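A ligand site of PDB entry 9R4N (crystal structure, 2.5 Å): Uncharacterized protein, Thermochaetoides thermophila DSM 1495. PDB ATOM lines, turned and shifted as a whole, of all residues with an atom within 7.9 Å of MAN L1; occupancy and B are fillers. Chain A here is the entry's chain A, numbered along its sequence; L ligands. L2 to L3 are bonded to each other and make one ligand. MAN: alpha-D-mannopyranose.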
ATOM      1  N   VAL A 210     -26.599  -6.260  -4.822  1.00  0.00           N
ATOM      2  CA  VAL A 210     -25.807  -6.501  -3.625  1.00  0.00           C
ATOM      3  C   VAL A 210     -26.686  -6.500  -2.368  1.00  0.00           C
ATOM      4  O   VAL A 210     -26.461  -7.288  -1.458  1.00  0.00           O
ATOM      5  CB  VAL A 210     -24.662  -5.468  -3.518  1.00  0.00           C
ATOM      6  CG1 VAL A 210     -25.208  -4.044  -3.465  1.00  0.00           C
ATOM      7  CG2 VAL A 210     -23.779  -5.768  -2.313  1.00  0.00           C
ATOM      8  N   ASP A 211     -27.698  -5.635  -2.334  1.00  0.00           N
ATOM      9  CA  ASP A 211     -28.627  -5.556  -1.203  1.00  0.00           C
ATOM     10  C   ASP A 211     -29.783  -6.500  -1.478  1.00  0.00           C
ATOM     11  O   ASP A 211     -30.711  -6.164  -2.223  1.00  0.00           O
ATOM     12  CB  ASP A 211     -29.105  -4.126  -0.986  1.00  0.00           C
ATOM     13  CG  ASP A 211     -29.392  -3.394  -2.286  1.00  0.00           C
ATOM     14  OD1 ASP A 211     -30.035  -2.325  -2.241  1.00  0.00           O
ATOM     15  OD2 ASP A 211     -28.959  -3.882  -3.351  1.00  0.00           O
ATOM     16  N   LEU A 215     -32.696  -4.486  -3.075  1.00  0.00           N
ATOM     17  CA  LEU A 215     -32.546  -4.556  -4.530  1.00  0.00           C
ATOM     18  C   LEU A 215     -32.561  -3.157  -5.158  1.00  0.00           C
ATOM     19  O   LEU A 215     -33.413  -2.806  -5.974  1.00  0.00           O
ATOM     20  CB  LEU A 215     -33.639  -5.439  -5.148  1.00  0.00           C
ATOM     21  CG  LEU A 215     -33.846  -6.825  -4.526  1.00  0.00           C
ATOM     22  CD1 LEU A 215     -34.921  -7.593  -5.276  1.00  0.00           C
ATOM     23  CD2 LEU A 215     -32.549  -7.595  -4.511  1.00  0.00           C
ATOM     24  N   THR A 216     -31.571  -2.349  -4.747  1.00  0.00           N
ATOM     25  CA  THR A 216     -31.446  -0.985  -5.254  1.00  0.00           C
ATOM     26  C   THR A 216     -30.052  -0.663  -5.784  1.00  0.00           C
ATOM     27  O   THR A 216     -29.834   0.473  -6.206  1.00  0.00           O
ATOM     28  CB  THR A 216     -31.807   0.030  -4.167  1.00  0.00           C
ATOM     29  OG1 THR A 216     -30.858  -0.057  -3.091  1.00  0.00           O
ATOM     30  CG2 THR A 216     -33.212  -0.219  -3.620  1.00  0.00           C
ATOM     31  N   TYR A 217     -29.122  -1.615  -5.777  1.00  0.00           N
ATOM     32  CA  TYR A 217     -27.745  -1.317  -6.153  1.00  0.00           C
ATOM     33  C   TYR A 217     -27.125  -2.542  -6.815  1.00  0.00           C
ATOM     34  O   TYR A 217     -27.083  -3.615  -6.220  1.00  0.00           O
ATOM     35  CB  TYR A 217     -26.923  -0.903  -4.928  1.00  0.00           C
ATOM     36  CG  TYR A 217     -25.631  -0.198  -5.258  1.00  0.00           C
ATOM     37  CD1 TYR A 217     -25.376   0.300  -6.532  1.00  0.00           C
ATOM     38  CD2 TYR A 217     -24.645  -0.029  -4.295  1.00  0.00           C
ATOM     39  CE1 TYR A 217     -24.190   0.938  -6.839  1.00  0.00           C
ATOM     40  CE2 TYR A 217     -23.452   0.613  -4.582  1.00  0.00           C
ATOM     41  CZ  TYR A 217     -23.239   1.099  -5.856  1.00  0.00           C
ATOM     42  OH  TYR A 217     -22.057   1.731  -6.151  1.00  0.00           O
ATOM     43  N   LYS A 218     -26.651  -2.364  -8.045  1.00  0.00           N
ATOM     44  CA  LYS A 218     -25.815  -3.354  -8.733  1.00  0.00           C
ATOM     45  C   LYS A 218     -24.408  -2.759  -8.792  1.00  0.00           C
ATOM     46  O   LYS A 218     -24.048  -2.079  -9.757  1.00  0.00           O
ATOM     47  CB  LYS A 218     -26.359  -3.664 -10.124  1.00  0.00           C
ATOM     48  CG  LYS A 218     -27.726  -4.331 -10.132  1.00  0.00           C
ATOM     49  CD  LYS A 218     -28.019  -4.915 -11.512  1.00  0.00           C
ATOM     50  CE  LYS A 218     -29.333  -5.686 -11.511  1.00  0.00           C
ATOM     51  NZ  LYS A 218     -29.537  -6.402 -12.807  1.00  0.00           N
ATOM     52  N   ASN A 219     -23.624  -3.005  -7.754  1.00  0.00           N
ATOM     53  CA  ASN A 219     -22.295  -2.418  -7.648  1.00  0.00           C
ATOM     54  C   ASN A 219     -21.268  -3.309  -8.339  1.00  0.00           C
ATOM     55  O   ASN A 219     -21.586  -4.332  -8.951  1.00  0.00           O
ATOM     56  CB  ASN A 219     -21.924  -2.167  -6.192  1.00  0.00           C
ATOM     57  CG  ASN A 219     -21.952  -3.436  -5.347  1.00  0.00           C
ATOM     58  OD1 ASN A 219     -22.135  -4.540  -5.854  1.00  0.00           O
ATOM     59  ND2 ASN A 219     -21.767  -3.269  -4.040  1.00  0.00           N
ATOM     60  N   ASP A 268     -17.299   2.380  -8.565  1.00  0.00           N
ATOM     61  CA  ASP A 268     -17.882   1.551  -7.509  1.00  0.00           C
ATOM     62  C   ASP A 268     -19.121   0.800  -7.974  1.00  0.00           C
ATOM     63  O   ASP A 268     -19.317  -0.365  -7.594  1.00  0.00           O
ATOM     64  CB  ASP A 268     -18.226   2.410  -6.295  1.00  0.00           C
ATOM     65  CG  ASP A 268     -18.588   1.571  -5.087  1.00  0.00           C
ATOM     66  OD1 ASP A 268     -17.693   0.867  -4.583  1.00  0.00           O
ATOM     67  OD2 ASP A 268     -19.756   1.597  -4.661  1.00  0.00           O
ATOM     68  N   GLY A 269     -19.984   1.415  -8.774  1.00  0.00           N
ATOM     69  CA  GLY A 269     -21.213   0.756  -9.142  1.00  0.00           C
ATOM     70  C   GLY A 269     -21.932   1.439 -10.277  1.00  0.00           C
ATOM     71  O   GLY A 269     -21.352   2.211 -11.039  1.00  0.00           O
ATOM     72  N   LEU A 270     -23.227   1.134 -10.378  1.00  0.00           N
ATOM     73  CA  LEU A 270     -24.079   1.631 -11.444  1.00  0.00           C
ATOM     74  C   LEU A 270     -25.235   2.440 -10.865  1.00  0.00           C
ATOM     75  O   LEU A 270     -25.704   2.181  -9.756  1.00  0.00           O
ATOM     76  CB  LEU A 270     -24.638   0.479 -12.290  1.00  0.00           C
ATOM     77  CG  LEU A 270     -23.687  -0.196 -13.262  1.00  0.00           C
ATOM     78  CD1 LEU A 270     -24.322  -1.474 -13.809  1.00  0.00           C
ATOM     79  CD2 LEU A 270     -23.308   0.747 -14.398  1.00  0.00           C
ATOM     80  N   ALA A 271     -25.684   3.425 -11.641  1.00  0.00           N
ATOM     81  CA  ALA A 271     -26.856   4.225 -11.304  1.00  0.00           C
ATOM     82  C   ALA A 271     -27.907   4.040 -12.395  1.00  0.00           C
ATOM     83  O   ALA A 271     -27.572   3.809 -13.556  1.00  0.00           O
ATOM     84  CB  ALA A 271     -26.496   5.702 -11.158  1.00  0.00           C
ATOM     85  N   ARG A 272     -29.169   4.149 -12.006  1.00  0.00           N
ATOM     86  CA  ARG A 272     -30.283   3.938 -12.915  1.00  0.00           C
ATOM     87  C   ARG A 272     -30.935   5.266 -13.275  1.00  0.00           C
ATOM     88  O   ARG A 272     -31.176   6.113 -12.406  1.00  0.00           O
ATOM     89  CB  ARG A 272     -31.327   3.003 -12.303  1.00  0.00           C
ATOM     90  CG  ARG A 272     -31.877   1.980 -13.276  1.00  0.00           C
ATOM     91  CD  ARG A 272     -33.364   1.744 -13.048  1.00  0.00           C
ATOM     92  NE  ARG A 272     -33.900   0.737 -13.962  1.00  0.00           N
ATOM     93  CZ  ARG A 272     -35.186   0.486 -14.122  1.00  0.00           C
ATOM     94  NH1 ARG A 272     -36.112   1.158 -13.453  1.00  0.00           N
ATOM     95  NH2 ARG A 272     -35.567  -0.460 -14.977  1.00  0.00           N
ATOM     96  N   TYR A 280     -25.927   3.467 -15.830  1.00  0.00           N
ATOM     97  CA  TYR A 280     -24.686   4.139 -16.197  1.00  0.00           C
ATOM     98  C   TYR A 280     -23.745   4.189 -14.997  1.00  0.00           C
ATOM     99  O   TYR A 280     -24.162   4.026 -13.851  1.00  0.00           O
ATOM    100  CB  TYR A 280     -24.947   5.553 -16.737  1.00  0.00           C
ATOM    101  CG  TYR A 280     -25.759   6.422 -15.805  1.00  0.00           C
ATOM    102  CD1 TYR A 280     -25.140   7.187 -14.824  1.00  0.00           C
ATOM    103  CD2 TYR A 280     -27.136   6.486 -15.910  1.00  0.00           C
ATOM    104  CE1 TYR A 280     -25.870   7.983 -13.966  1.00  0.00           C
ATOM    105  CE2 TYR A 280     -27.886   7.285 -15.055  1.00  0.00           C
ATOM    106  CZ  TYR A 280     -27.247   8.031 -14.087  1.00  0.00           C
ATOM    107  OH  TYR A 280     -27.986   8.826 -13.239  1.00  0.00           O
ATOM    108  N   ASN A 281     -22.465   4.402 -15.302  1.00  0.00           N
ATOM    109  CA  ASN A 281     -21.451   4.555 -14.268  1.00  0.00           C
ATOM    110  C   ASN A 281     -21.822   5.690 -13.317  1.00  0.00           C
ATOM    111  O   ASN A 281     -22.067   6.817 -13.739  1.00  0.00           O
ATOM    112  CB  ASN A 281     -20.093   4.840 -14.938  1.00  0.00           C
ATOM    113  CG  ASN A 281     -18.936   4.806 -13.964  1.00  0.00           C
ATOM    114  OD1 ASN A 281     -18.987   5.390 -12.883  1.00  0.00           O
ATOM    115  ND2 ASN A 281     -17.855   4.143 -14.366  1.00  0.00           N
ATOM    116  N   ASN A 282     -21.845   5.385 -12.021  1.00  0.00           N
ATOM    117  CA  ASN A 282     -22.220   6.368 -11.010  1.00  0.00           C
ATOM    118  C   ASN A 282     -21.074   7.263 -10.591  1.00  0.00           C
ATOM    119  O   ASN A 282     -21.280   8.165  -9.759  1.00  0.00           O
ATOM    120  CB  ASN A 282     -22.810   5.673  -9.767  1.00  0.00           C
ATOM    121  CG  ASN A 282     -21.870   4.650  -9.162  1.00  0.00           C
ATOM    122  OD1 ASN A 282     -20.701   4.555  -9.534  1.00  0.00           O
ATOM    123  ND2 ASN A 282     -22.377   3.881  -8.204  1.00  0.00           N
ATOM    124  N   ARG A 283     -19.870   7.047 -11.120  1.00  0.00           N
ATOM    125  CA  ARG A 283     -18.701   7.884 -10.839  1.00  0.00           C
ATOM    126  C   ARG A 283     -18.379   7.929  -9.350  1.00  0.00           C
ATOM    127  O   ARG A 283     -17.864   8.932  -8.840  1.00  0.00           O
ATOM    128  CB  ARG A 283     -18.889   9.299 -11.394  1.00  0.00           C
ATOM    129  CG  ARG A 283     -19.229   9.333 -12.879  1.00  0.00           C
ATOM    130  CD  ARG A 283     -18.154   8.661 -13.724  1.00  0.00           C
ATOM    131  NE  ARG A 283     -18.666   8.205 -15.009  1.00  0.00           N
ATOM    132  CZ  ARG A 283     -17.906   7.775 -16.008  1.00  0.00           C
ATOM    133  NH1 ARG A 283     -16.594   7.744 -15.910  1.00  0.00           N
ATOM    134  NH2 ARG A 283     -18.485   7.372 -17.138  1.00  0.00           N
ATOM    135  N   LEU A 284     -18.674   6.847  -8.637  1.00  0.00           N
ATOM    136  CA  LEU A 284     -18.334   6.735  -7.231  1.00  0.00           C
ATOM    137  C   LEU A 284     -16.854   6.378  -7.103  1.00  0.00           C
ATOM    138  O   LEU A 284     -16.208   6.021  -8.085  1.00  0.00           O
ATOM    139  CB  LEU A 284     -19.238   5.699  -6.573  1.00  0.00           C
ATOM    140  CG  LEU A 284     -20.363   6.282  -5.704  1.00  0.00           C
ATOM    141  CD1 LEU A 284     -21.129   7.349  -6.464  1.00  0.00           C
ATOM    142  CD2 LEU A 284     -21.292   5.190  -5.208  1.00  0.00           C
HETATM  143  C1  MAN L   1     -26.060   4.540  -4.066  1.00  0.00           C
HETATM  144  C2  MAN L   1     -26.711   3.130  -3.988  1.00  0.00           C
HETATM  145  C3  MAN L   1     -27.681   2.860  -5.159  1.00  0.00           C
HETATM  146  C4  MAN L   1     -27.496   3.876  -6.295  1.00  0.00           C
HETATM  147  C5  MAN L   1     -26.012   4.137  -6.479  1.00  0.00           C
HETATM  148  C6  MAN L   1     -25.710   4.961  -7.709  1.00  0.00           C
HETATM  149  O1  MAN L   1     -25.072   4.573  -3.058  1.00  0.00           O
HETATM  150  O2  MAN L   1     -27.491   2.983  -2.798  1.00  0.00           O
HETATM  151  O3  MAN L   1     -29.042   2.831  -4.733  1.00  0.00           O
HETATM  152  O4  MAN L   1     -28.049   3.368  -7.504  1.00  0.00           O
HETATM  153  O5  MAN L   1     -25.523   4.885  -5.335  1.00  0.00           O
HETATM  154  O6  MAN L   1     -26.153   6.301  -7.481  1.00  0.00           O
HETATM  155  C1  MAN L   2     -20.186  -0.513   0.597  1.00  0.00           C
HETATM  156  C2  MAN L   2     -20.673  -0.346  -0.799  1.00  0.00           C
HETATM  157  C3  MAN L   2     -19.647  -0.729  -1.744  1.00  0.00           C
HETATM  158  C4  MAN L   2     -18.440   0.104  -1.585  1.00  0.00           C
HETATM  159  C5  MAN L   2     -17.852   0.035  -0.148  1.00  0.00           C
HETATM  160  C6  MAN L   2     -16.863   1.024  -0.010  1.00  0.00           C
HETATM  161  O1  MAN L   2     -19.874  -1.858   0.813  1.00  0.00           O
HETATM  162  O2  MAN L   2     -20.988   1.105  -1.018  1.00  0.00           O
HETATM  163  O3  MAN L   2     -20.178  -0.571  -3.131  1.00  0.00           O
HETATM  164  O4  MAN L   2     -17.439  -0.344  -2.512  1.00  0.00           O
HETATM  165  O5  MAN L   2     -18.987   0.297   0.848  1.00  0.00           O
HETATM  166  O6  MAN L   2     -16.701   1.354   1.357  1.00  0.00           O
HETATM  167  C1  MAN L   3     -22.382   1.371  -0.864  1.00  0.00           C
HETATM  168  C2  MAN L   3     -22.693   2.602  -1.613  1.00  0.00           C
HETATM  169  C3  MAN L   3     -22.080   3.763  -0.976  1.00  0.00           C
HETATM  170  C4  MAN L   3     -22.610   4.040   0.372  1.00  0.00           C
HETATM  171  C5  MAN L   3     -23.027   2.794   1.234  1.00  0.00           C
HETATM  172  C6  MAN L   3     -24.404   2.841   1.516  1.00  0.00           C
HETATM  173  O2  MAN L   3     -24.163   2.793  -1.717  1.00  0.00           O
HETATM  174  O3  MAN L   3     -22.330   4.960  -1.825  1.00  0.00           O
HETATM  175  O4  MAN L   3     -21.580   4.767   1.099  1.00  0.00           O
HETATM  176  O5  MAN L   3     -22.675   1.436   0.578  1.00  0.00           O
HETATM  177  O6  MAN L   3     -24.828   4.195   1.699  1.00  0.00           O
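O3 of MAN L2 is in hydrogen-bond range of ND2 of Asn 219 (3.3 Å).
The backbone carbonyl oxygen of Leu 270 sits close to an oxygen (O4) of MAN L1 (3.5 Å).
An oxygen (O4) of MAN L2 lies within hydrogen-bond range of the side-chain carboxylate of Asp 268 (2.4 Å).
O of Thr 216 sits at hydrogen-bond distance from O3 of MAN L1.
An oxygen (O2) of MAN L3 is in hydrogen-bond range of an oxygen (O1) of MAN L1, 2.4 Å away.
O of Lys 218 lies within hydrogen-bond range of N of Leu 270, 3.4 Å away.
The backbone NH of Tyr 217 lies within hydrogen-bond range of the side-chain carboxylate of Asp 211 (3.3 Å).
The side-chain hydroxyl (OG1) of Thr 216 lies within hydrogen-bond range of the side-chain carboxylate (OD1) of Asp 211.
O of Tyr 217 is in hydrogen-bond range of N of Val 210, 3.0 Å away.
N of Leu 284 sits close to OD1 of Asn 282 (3.2 Å).
The side-chain hydroxyl of Tyr 217 sits at hydrogen-bond distance from the side-chain amide nitrogen of Asn 282, at 3.0 Å.
The side-chain carboxylate of Asp 268 lies within hydrogen-bond range of the side-chain hydroxyl of Tyr 217 (2.7 Å).
O of Tyr 280 sits at hydrogen-bond distance from N of Ala 271.
Tyr 217 touches MAN L1 (CG to C3, 3.7 Å).
Ala 271 touches MAN L1.
Asn 282 touches MAN L1 (ND2 to C6, 3.5 Å).
Of the 17 residues printed, 5 come within 4 Å of MAN L1.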
